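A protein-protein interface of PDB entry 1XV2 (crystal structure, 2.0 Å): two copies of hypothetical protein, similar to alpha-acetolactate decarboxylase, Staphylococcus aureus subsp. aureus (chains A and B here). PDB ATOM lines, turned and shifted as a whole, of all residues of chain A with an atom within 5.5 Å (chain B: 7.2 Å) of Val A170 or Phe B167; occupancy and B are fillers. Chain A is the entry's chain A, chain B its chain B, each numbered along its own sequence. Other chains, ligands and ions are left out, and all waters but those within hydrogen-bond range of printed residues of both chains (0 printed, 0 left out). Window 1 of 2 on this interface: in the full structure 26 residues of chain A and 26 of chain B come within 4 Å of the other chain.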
ATOM      1  N   GLN A  10      11.766 -19.025 -12.448  1.00  0.00           N
ATOM      2  CA  GLN A  10      11.829 -17.642 -12.017  1.00  0.00           C
ATOM      3  C   GLN A  10      12.661 -17.502 -10.749  1.00  0.00           C
ATOM      4  O   GLN A  10      12.490 -18.252  -9.786  1.00  0.00           O
ATOM      5  CB  GLN A  10      10.418 -17.078 -11.796  1.00  0.00           C
ATOM      6  CG  GLN A  10      10.396 -15.589 -11.466  1.00  0.00           C
ATOM      7  CD  GLN A  10       9.018 -14.955 -11.619  1.00  0.00           C
ATOM      8  OE1 GLN A  10       8.608 -14.584 -12.720  1.00  0.00           O
ATOM      9  NE2 GLN A  10       8.297 -14.832 -10.511  1.00  0.00           N
ATOM     10  N   GLY A  12      13.463 -15.002  -7.809  1.00  0.00           N
ATOM     11  CA  GLY A  12      12.956 -13.789  -7.197  1.00  0.00           C
ATOM     12  C   GLY A  12      11.599 -13.500  -7.801  1.00  0.00           C
ATOM     13  O   GLY A  12      11.111 -14.278  -8.627  1.00  0.00           O
ATOM     14  N   THR A  13      10.984 -12.390  -7.407  1.00  0.00           N
ATOM     15  CA  THR A  13       9.666 -12.033  -7.924  1.00  0.00           C
ATOM     16  C   THR A  13       9.579 -10.557  -8.297  1.00  0.00           C
ATOM     17  O   THR A  13      10.404  -9.748  -7.878  1.00  0.00           O
ATOM     18  CB  THR A  13       8.566 -12.344  -6.889  1.00  0.00           C
ATOM     19  OG1 THR A  13       8.784 -11.556  -5.714  1.00  0.00           O
ATOM     20  CG2 THR A  13       8.594 -13.813  -6.501  1.00  0.00           C
ATOM     21  N   LEU A  14       8.572 -10.207  -9.089  1.00  0.00           N
ATOM     22  CA  LEU A  14       8.392  -8.824  -9.508  1.00  0.00           C
ATOM     23  C   LEU A  14       7.950  -7.942  -8.345  1.00  0.00           C
ATOM     24  O   LEU A  14       8.417  -6.817  -8.199  1.00  0.00           O
ATOM     25  CB  LEU A  14       7.363  -8.743 -10.635  1.00  0.00           C
ATOM     26  CG  LEU A  14       7.054  -7.336 -11.154  1.00  0.00           C
ATOM     27  CD1 LEU A  14       8.334  -6.676 -11.636  1.00  0.00           C
ATOM     28  CD2 LEU A  14       6.032  -7.422 -12.272  1.00  0.00           C
ATOM     29  N   GLY A  15       7.054  -8.464  -7.516  1.00  0.00           N
ATOM     30  CA  GLY A  15       6.565  -7.703  -6.381  1.00  0.00           C
ATOM     31  C   GLY A  15       7.640  -7.331  -5.373  1.00  0.00           C
ATOM     32  O   GLY A  15       7.629  -6.226  -4.837  1.00  0.00           O
ATOM     33  N   TYR A  76      16.150 -10.324 -10.100  1.00  0.00           N
ATOM     34  CA  TYR A  76      14.909 -10.893 -10.621  1.00  0.00           C
ATOM     35  C   TYR A  76      15.080 -11.347 -12.066  1.00  0.00           C
ATOM     36  O   TYR A  76      15.515 -10.578 -12.918  1.00  0.00           O
ATOM     37  CB  TYR A  76      13.775  -9.865 -10.544  1.00  0.00           C
ATOM     38  CG  TYR A  76      12.460 -10.367 -11.109  1.00  0.00           C
ATOM     39  CD1 TYR A  76      11.963 -11.621 -10.757  1.00  0.00           C
ATOM     40  CD2 TYR A  76      11.710  -9.584 -11.983  1.00  0.00           C
ATOM     41  CE1 TYR A  76      10.753 -12.085 -11.262  1.00  0.00           C
ATOM     42  CE2 TYR A  76      10.492 -10.037 -12.494  1.00  0.00           C
ATOM     43  CZ  TYR A  76      10.022 -11.289 -12.129  1.00  0.00           C
ATOM     44  OH  TYR A  76       8.823 -11.752 -12.629  1.00  0.00           O
ATOM     45  N   PHE A 167      -1.487 -14.978 -10.423  1.00  0.00           N
ATOM     46  CA  PHE A 167      -0.068 -14.843 -10.144  1.00  0.00           C
ATOM     47  C   PHE A 167       0.469 -13.427 -10.320  1.00  0.00           C
ATOM     48  O   PHE A 167       1.678 -13.203 -10.283  1.00  0.00           O
ATOM     49  CB  PHE A 167       0.711 -15.837 -11.005  1.00  0.00           C
ATOM     50  CG  PHE A 167       0.632 -17.247 -10.501  1.00  0.00           C
ATOM     51  CD1 PHE A 167       1.584 -17.734  -9.608  1.00  0.00           C
ATOM     52  CD2 PHE A 167      -0.412 -18.082 -10.887  1.00  0.00           C
ATOM     53  CE1 PHE A 167       1.494 -19.031  -9.106  1.00  0.00           C
ATOM     54  CE2 PHE A 167      -0.508 -19.380 -10.391  1.00  0.00           C
ATOM     55  CZ  PHE A 167       0.447 -19.854  -9.499  1.00  0.00           C
ATOM     56  N   HIS A 168      -0.428 -12.468 -10.504  1.00  0.00           N
ATOM     57  CA  HIS A 168      -0.006 -11.081 -10.645  1.00  0.00           C
ATOM     58  C   HIS A 168       0.711 -10.686  -9.351  1.00  0.00           C
ATOM     59  O   HIS A 168       0.172 -10.851  -8.258  1.00  0.00           O
ATOM     60  CB  HIS A 168      -1.221 -10.177 -10.890  1.00  0.00           C
ATOM     61  CG  HIS A 168      -1.826 -10.337 -12.254  1.00  0.00           C
ATOM     62  ND1 HIS A 168      -2.938  -9.629 -12.662  1.00  0.00           N
ATOM     63  CD2 HIS A 168      -1.459 -11.101 -13.310  1.00  0.00           C
ATOM     64  CE1 HIS A 168      -3.227  -9.949 -13.912  1.00  0.00           C
ATOM     65  NE2 HIS A 168      -2.345 -10.840 -14.328  1.00  0.00           N
ATOM     66  N   GLY A 169       1.931 -10.173  -9.478  1.00  0.00           N
ATOM     67  CA  GLY A 169       2.703  -9.803  -8.303  1.00  0.00           C
ATOM     68  C   GLY A 169       3.937 -10.685  -8.261  1.00  0.00           C
ATOM     69  O   GLY A 169       5.062 -10.193  -8.168  1.00  0.00           O
ATOM     70  N   VAL A 170       3.720 -11.996  -8.322  1.00  0.00           N
ATOM     71  CA  VAL A 170       4.818 -12.959  -8.339  1.00  0.00           C
ATOM     72  C   VAL A 170       5.481 -12.720  -9.688  1.00  0.00           C
ATOM     73  O   VAL A 170       6.705 -12.685  -9.813  1.00  0.00           O
ATOM     74  CB  VAL A 170       4.289 -14.412  -8.263  1.00  0.00           C
ATOM     75  CG1 VAL A 170       5.443 -15.406  -8.384  1.00  0.00           C
ATOM     76  CG2 VAL A 170       3.559 -14.618  -6.952  1.00  0.00           C
ATOM     77  N   GLY A 171       4.632 -12.543 -10.692  1.00  0.00           N
ATOM     78  CA  GLY A 171       5.085 -12.250 -12.037  1.00  0.00           C
ATOM     79  C   GLY A 171       4.441 -10.919 -12.377  1.00  0.00           C
ATOM     80  O   GLY A 171       4.098 -10.162 -11.471  1.00  0.00           O
ATOM     81  N   SER A 172       4.264 -10.621 -13.659  1.00  0.00           N
ATOM     82  CA  SER A 172       3.646  -9.357 -14.045  1.00  0.00           C
ATOM     83  C   SER A 172       2.252  -9.586 -14.611  1.00  0.00           C
ATOM     84  O   SER A 172       1.970 -10.627 -15.192  1.00  0.00           O
ATOM     85  CB  SER A 172       4.516  -8.629 -15.069  1.00  0.00           C
ATOM     86  OG  SER A 172       4.803  -9.464 -16.171  1.00  0.00           O
ATOM     87  N   PHE A 208       5.660 -24.208 -12.965  1.00  0.00           N
ATOM     88  CA  PHE A 208       6.261 -22.915 -12.663  1.00  0.00           C
ATOM     89  C   PHE A 208       7.208 -23.157 -11.493  1.00  0.00           C
ATOM     90  O   PHE A 208       6.771 -23.521 -10.402  1.00  0.00           O
ATOM     91  CB  PHE A 208       5.170 -21.923 -12.256  1.00  0.00           C
ATOM     92  CG  PHE A 208       5.689 -20.592 -11.794  1.00  0.00           C
ATOM     93  CD1 PHE A 208       6.330 -19.733 -12.677  1.00  0.00           C
ATOM     94  CD2 PHE A 208       5.514 -20.188 -10.474  1.00  0.00           C
ATOM     95  CE1 PHE A 208       6.790 -18.486 -12.249  1.00  0.00           C
ATOM     96  CE2 PHE A 208       5.971 -18.945 -10.039  1.00  0.00           C
ATOM     97  CZ  PHE A 208       6.608 -18.094 -10.927  1.00  0.00           C
ATOM     98  N   GLN A 210       9.607 -21.536  -8.891  1.00  0.00           N
ATOM     99  CA  GLN A 210      10.011 -20.293  -8.232  1.00  0.00           C
ATOM    100  C   GLN A 210      11.180 -20.510  -7.275  1.00  0.00           C
ATOM    101  O   GLN A 210      11.086 -21.304  -6.341  1.00  0.00           O
ATOM    102  CB  GLN A 210       8.829 -19.698  -7.459  1.00  0.00           C
ATOM    103  CG  GLN A 210       9.164 -18.431  -6.680  1.00  0.00           C
ATOM    104  CD  GLN A 210       9.489 -17.255  -7.582  1.00  0.00           C
ATOM    105  OE1 GLN A 210       8.610 -16.718  -8.259  1.00  0.00           O
ATOM    106  NE2 GLN A 210      10.754 -16.852  -7.600  1.00  0.00           N
ATOM    107  N   PHE A 212      14.032 -18.849  -4.568  1.00  0.00           N
ATOM    108  CA  PHE A 212      14.231 -17.759  -3.620  1.00  0.00           C
ATOM    109  C   PHE A 212      15.687 -17.685  -3.153  1.00  0.00           C
ATOM    110  O   PHE A 212      16.335 -18.711  -2.961  1.00  0.00           O
ATOM    111  CB  PHE A 212      13.339 -17.970  -2.389  1.00  0.00           C
ATOM    112  CG  PHE A 212      11.862 -17.979  -2.690  1.00  0.00           C
ATOM    113  CD1 PHE A 212      11.085 -16.847  -2.456  1.00  0.00           C
ATOM    114  CD2 PHE A 212      11.246 -19.124  -3.190  1.00  0.00           C
ATOM    115  CE1 PHE A 212       9.714 -16.852  -2.714  1.00  0.00           C
ATOM    116  CE2 PHE A 212       9.872 -19.141  -3.452  1.00  0.00           C
ATOM    117  CZ  PHE A 212       9.106 -18.002  -3.213  1.00  0.00           C
ATOM    118  N   GLN B  10       3.312 -28.047  -5.150  1.00  0.00           N
ATOM    119  CA  GLN B  10       1.900 -27.719  -5.050  1.00  0.00           C
ATOM    120  C   GLN B  10       1.182 -27.939  -6.379  1.00  0.00           C
ATOM    121  O   GLN B  10       1.605 -27.439  -7.421  1.00  0.00           O
ATOM    122  CB  GLN B  10       1.727 -26.270  -4.585  1.00  0.00           C
ATOM    123  CG  GLN B  10       0.282 -25.839  -4.425  1.00  0.00           C
ATOM    124  CD  GLN B  10       0.141 -24.466  -3.784  1.00  0.00           C
ATOM    125  OE1 GLN B  10       0.250 -24.318  -2.568  1.00  0.00           O
ATOM    126  NE2 GLN B  10      -0.102 -23.455  -4.606  1.00  0.00           N
ATOM    127  N   ASN B 110       9.492 -14.309   4.552  1.00  0.00           N
ATOM    128  CA  ASN B 110       9.396 -13.992   3.129  1.00  0.00           C
ATOM    129  C   ASN B 110       9.576 -15.251   2.277  1.00  0.00           C
ATOM    130  O   ASN B 110       9.602 -15.190   1.047  1.00  0.00           O
ATOM    131  CB  ASN B 110      10.444 -12.938   2.751  1.00  0.00           C
ATOM    132  CG  ASN B 110      10.331 -11.682   3.602  1.00  0.00           C
ATOM    133  OD1 ASN B 110       9.232 -11.196   3.864  1.00  0.00           O
ATOM    134  ND2 ASN B 110      11.470 -11.148   4.034  1.00  0.00           N
ATOM    135  N   LEU B 111       9.688 -16.390   2.953  1.00  0.00           N
ATOM    136  CA  LEU B 111       9.855 -17.688   2.307  1.00  0.00           C
ATOM    137  C   LEU B 111       8.710 -18.619   2.670  1.00  0.00           C
ATOM    138  O   LEU B 111       7.985 -18.379   3.634  1.00  0.00           O
ATOM    139  CB  LEU B 111      11.153 -18.361   2.780  1.00  0.00           C
ATOM    140  CG  LEU B 111      12.521 -17.769   2.438  1.00  0.00           C
ATOM    141  CD1 LEU B 111      13.598 -18.503   3.228  1.00  0.00           C
ATOM    142  CD2 LEU B 111      12.778 -17.896   0.944  1.00  0.00           C
ATOM    143  N   PHE B 112       8.558 -19.684   1.892  1.00  0.00           N
ATOM    144  CA  PHE B 112       7.562 -20.704   2.181  1.00  0.00           C
ATOM    145  C   PHE B 112       8.286 -21.601   3.180  1.00  0.00           C
ATOM    146  O   PHE B 112       9.516 -21.694   3.149  1.00  0.00           O
ATOM    147  CB  PHE B 112       7.262 -21.553   0.947  1.00  0.00           C
ATOM    148  CG  PHE B 112       6.282 -20.944  -0.006  1.00  0.00           C
ATOM    149  CD1 PHE B 112       4.917 -21.124   0.175  1.00  0.00           C
ATOM    150  CD2 PHE B 112       6.725 -20.232  -1.119  1.00  0.00           C
ATOM    151  CE1 PHE B 112       4.008 -20.611  -0.741  1.00  0.00           C
ATOM    152  CE2 PHE B 112       5.819 -19.713  -2.043  1.00  0.00           C
ATOM    153  CZ  PHE B 112       4.461 -19.907  -1.853  1.00  0.00           C
ATOM    154  N   THR B 163       2.853 -19.558   4.071  1.00  0.00           N
ATOM    155  CA  THR B 163       2.957 -18.909   2.773  1.00  0.00           C
ATOM    156  C   THR B 163       3.298 -17.432   2.957  1.00  0.00           C
ATOM    157  O   THR B 163       2.609 -16.714   3.679  1.00  0.00           O
ATOM    158  CB  THR B 163       1.630 -19.025   1.993  1.00  0.00           C
ATOM    159  OG1 THR B 163       1.317 -20.408   1.786  1.00  0.00           O
ATOM    160  CG2 THR B 163       1.742 -18.333   0.640  1.00  0.00           C
ATOM    161  N   PRO B 164       4.377 -16.963   2.309  1.00  0.00           N
ATOM    162  CA  PRO B 164       4.771 -15.557   2.434  1.00  0.00           C
ATOM    163  C   PRO B 164       3.683 -14.650   1.845  1.00  0.00           C
ATOM    164  O   PRO B 164       2.902 -15.084   0.996  1.00  0.00           O
ATOM    165  CB  PRO B 164       6.094 -15.506   1.674  1.00  0.00           C
ATOM    166  CG  PRO B 164       5.908 -16.546   0.604  1.00  0.00           C
ATOM    167  CD  PRO B 164       5.245 -17.679   1.354  1.00  0.00           C
ATOM    168  N   GLU B 165       3.644 -13.397   2.290  1.00  0.00           N
ATOM    169  CA  GLU B 165       2.620 -12.448   1.850  1.00  0.00           C
ATOM    170  C   GLU B 165       2.333 -12.344   0.354  1.00  0.00           C
ATOM    171  O   GLU B 165       1.186 -12.467  -0.063  1.00  0.00           O
ATOM    172  CB  GLU B 165       2.928 -11.045   2.370  1.00  0.00           C
ATOM    173  CG  GLU B 165       1.748 -10.093   2.216  1.00  0.00           C
ATOM    174  CD  GLU B 165       2.101  -8.641   2.479  1.00  0.00           C
ATOM    175  OE1 GLU B 165       2.815  -8.363   3.467  1.00  0.00           O
ATOM    176  OE2 GLU B 165       1.647  -7.774   1.700  1.00  0.00           O
ATOM    177  N   LEU B 166       3.363 -12.103  -0.450  1.00  0.00           N
ATOM    178  CA  LEU B 166       3.183 -11.949  -1.893  1.00  0.00           C
ATOM    179  C   LEU B 166       2.505 -13.143  -2.560  1.00  0.00           C
ATOM    180  O   LEU B 166       1.917 -13.012  -3.637  1.00  0.00           O
ATOM    181  CB  LEU B 166       4.533 -11.691  -2.565  1.00  0.00           C
ATOM    182  CG  LEU B 166       4.497 -11.325  -4.054  1.00  0.00           C
ATOM    183  CD1 LEU B 166       3.787  -9.993  -4.240  1.00  0.00           C
ATOM    184  CD2 LEU B 166       5.921 -11.238  -4.588  1.00  0.00           C
ATOM    185  N   PHE B 167       2.576 -14.305  -1.924  1.00  0.00           N
ATOM    186  CA  PHE B 167       1.968 -15.500  -2.489  1.00  0.00           C
ATOM    187  C   PHE B 167       0.566 -15.804  -1.952  1.00  0.00           C
ATOM    188  O   PHE B 167       0.005 -16.862  -2.230  1.00  0.00           O
ATOM    189  CB  PHE B 167       2.899 -16.697  -2.278  1.00  0.00           C
ATOM    190  CG  PHE B 167       4.106 -16.687  -3.179  1.00  0.00           C
ATOM    191  CD1 PHE B 167       4.142 -17.470  -4.326  1.00  0.00           C
ATOM    192  CD2 PHE B 167       5.191 -15.861  -2.900  1.00  0.00           C
ATOM    193  CE1 PHE B 167       5.244 -17.432  -5.186  1.00  0.00           C
ATOM    194  CE2 PHE B 167       6.296 -15.815  -3.753  1.00  0.00           C
ATOM    195  CZ  PHE B 167       6.320 -16.600  -4.896  1.00  0.00           C
ATOM    196  N   HIS B 168      -0.006 -14.883  -1.184  1.00  0.00           N
ATOM    197  CA  HIS B 168      -1.353 -15.103  -0.667  1.00  0.00           C
ATOM    198  C   HIS B 168      -2.289 -15.210  -1.868  1.00  0.00           C
ATOM    199  O   HIS B 168      -2.361 -14.302  -2.689  1.00  0.00           O
ATOM    200  CB  HIS B 168      -1.775 -13.953   0.249  1.00  0.00           C
ATOM    201  CG  HIS B 168      -1.068 -13.949   1.570  1.00  0.00           C
ATOM    202  ND1 HIS B 168      -1.265 -12.967   2.518  1.00  0.00           N
ATOM    203  CD2 HIS B 168      -0.177 -14.817   2.107  1.00  0.00           C
ATOM    204  CE1 HIS B 168      -0.527 -13.232   3.583  1.00  0.00           C
ATOM    205  NE2 HIS B 168       0.142 -14.349   3.359  1.00  0.00           N
ATOM    206  N   GLY B 169      -2.988 -16.335  -1.970  1.00  0.00           N
ATOM    207  CA  GLY B 169      -3.882 -16.561  -3.092  1.00  0.00           C
ATOM    208  C   GLY B 169      -3.394 -17.804  -3.808  1.00  0.00           C
ATOM    209  O   GLY B 169      -4.162 -18.736  -4.060  1.00  0.00           O
ATOM    210  N   VAL B 170      -2.105 -17.809  -4.140  1.00  0.00           N
ATOM    211  CA  VAL B 170      -1.475 -18.954  -4.790  1.00  0.00           C
ATOM    212  C   VAL B 170      -1.500 -20.036  -3.716  1.00  0.00           C
ATOM    213  O   VAL B 170      -1.793 -21.204  -3.980  1.00  0.00           O
ATOM    214  CB  VAL B 170      -0.010 -18.625  -5.184  1.00  0.00           C
ATOM    215  CG1 VAL B 170       0.735 -19.893  -5.591  1.00  0.00           C
ATOM    216  CG2 VAL B 170      -0.002 -17.622  -6.329  1.00  0.00           C
ATOM    217  N   GLY B 171      -1.197 -19.605  -2.496  1.00  0.00           N
ATOM    218  CA  GLY B 171      -1.213 -20.472  -1.335  1.00  0.00           C
ATOM    219  C   GLY B 171      -2.101 -19.748  -0.342  1.00  0.00           C
ATOM    220  O   GLY B 171      -2.763 -18.784  -0.719  1.00  0.00           O
ATOM    221  N   SER B 172      -2.127 -20.181   0.916  1.00  0.00           N
ATOM    222  CA  SER B 172      -2.969 -19.515   1.905  1.00  0.00           C
ATOM    223  C   SER B 172      -2.273 -18.275   2.462  1.00  0.00           C
ATOM    224  O   SER B 172      -1.115 -18.010   2.147  1.00  0.00           O
ATOM    225  CB  SER B 172      -3.316 -20.476   3.041  1.00  0.00           C
ATOM    226  OG  SER B 172      -4.297 -19.909   3.894  1.00  0.00           O
ATOM    227  N   ALA B 173      -2.984 -17.511   3.284  1.00  0.00           N
ATOM    228  CA  ALA B 173      -2.424 -16.301   3.876  1.00  0.00           C
ATOM    229  C   ALA B 173      -1.771 -16.601   5.223  1.00  0.00           C
ATOM    230  O   ALA B 173      -2.371 -16.387   6.273  1.00  0.00           O
ATOM    231  CB  ALA B 173      -3.519 -15.253   4.041  1.00  0.00           C
ATOM    232  N   PHE B 208       9.846 -23.268  -4.895  1.00  0.00           N
ATOM    233  CA  PHE B 208       8.402 -23.486  -4.893  1.00  0.00           C
ATOM    234  C   PHE B 208       8.015 -24.028  -6.269  1.00  0.00           C
ATOM    235  O   PHE B 208       8.057 -23.308  -7.263  1.00  0.00           O
ATOM    236  CB  PHE B 208       7.674 -22.169  -4.607  1.00  0.00           C
ATOM    237  CG  PHE B 208       6.173 -22.274  -4.647  1.00  0.00           C
ATOM    238  CD1 PHE B 208       5.491 -23.087  -3.749  1.00  0.00           C
ATOM    239  CD2 PHE B 208       5.440 -21.554  -5.586  1.00  0.00           C
ATOM    240  CE1 PHE B 208       4.102 -23.182  -3.785  1.00  0.00           C
ATOM    241  CE2 PHE B 208       4.051 -21.642  -5.629  1.00  0.00           C
ATOM    242  CZ  PHE B 208       3.381 -22.458  -4.727  1.00  0.00           C
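O of Phe A208 sits close to O of Phe B208 (3.4 Å).
The backbone carbonyl oxygen (O) of Gln A210 lies within hydrogen-bond range of the backbone NH (N) of Phe B208.
NE2 of Gln A10 is in hydrogen-bond range of O of Val A170, at 2.8 Å.
O of Val A170 is in hydrogen-bond range of N of Leu A14.
NE2 of Gln A10 is in hydrogen-bond range of OE1 of Gln A210 (3.0 Å).
The side-chain amide nitrogen (NE2) of Gln A210 is in hydrogen-bond range of the backbone carbonyl oxygen (O) of Gly A12, 2.8 Å away.
The backbone carbonyl oxygen (O) of Gly A169 lies within hydrogen-bond range of the backbone NH (N) of Gly A15.
The side-chain amide nitrogen (NE2) of Gln B10 lies within hydrogen-bond range of the backbone carbonyl oxygen (O) of Val B170, at 2.9 Å.
OG1 of Thr A13 touches CD2 of Leu B166 (3.1 Å).
CZ of Phe B167 touches CG2 of Thr A13, 3.9 Å away.
Val B170 touches Phe A167 (CG2 to CE1, 3.5 Å).
Gly A169 touches Leu B166 (O to CD2, 3.8 Å).
Val A170 touches Phe B167 (CG2 to CE1, 3.7 Å).
Phe B167 touches Gln A210 (CZ to CG, 3.8 Å).
CB of Phe A212 touches CD2 of Leu B111, 3.4 Å away.
Phe B112 touches Phe A212 (CD2 to CZ, 3.9 Å).
Phe B167 touches Phe A212 (CZ to CZ, 3.5 Å).
Phe A212 touches Phe B208 (CE2 to CB, 3.9 Å).
Gly A12 touches none of the printed residues of chain B.
Printed residues of chain B within 4 Å of Phe A167: Val B170.
Gly A169 touches just one residue of chain B: Leu B166.
Val A170 touches just one residue of chain B: Phe B167 (3.7 Å).
Of the printed residues of chain A, Leu B111 touches Phe A212 (3.4 Å).
Of chain A, only Thr A13 (3.9 Å), Val A170 (3.7 Å), Gln A210 (3.8 Å) and Phe A212 (3.5 Å) come within 4 Å of Phe B167.
Gly B169 touches none of the printed residues of chain A.
The nearest residue of chain B that does not touch Val A170 is Leu B166 (4.03 Å).
Of the 16 printed residues of chain B, 6 touch a printed residue of chain A.
Along chain B the printed residues that touch a printed residue of chain A span positions 111 to 208.
Hydrophobic or aromatic side chains of chain A that line the printed part of chain B: Phe A167, Val A170 and Phe A212.
Phe A167 touches Val B170, and with the chains exchanged Val A170 touches Phe B167.
Phe A208 touches its own counterpart, Phe B208.
Positions printed for both chains: 10, 167, 168, 169, 170, 171, 172 and 208.
Of the 12 pairs that touch across the chains among the printed residues, 3 have their exchanged pair printed and touching as well.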
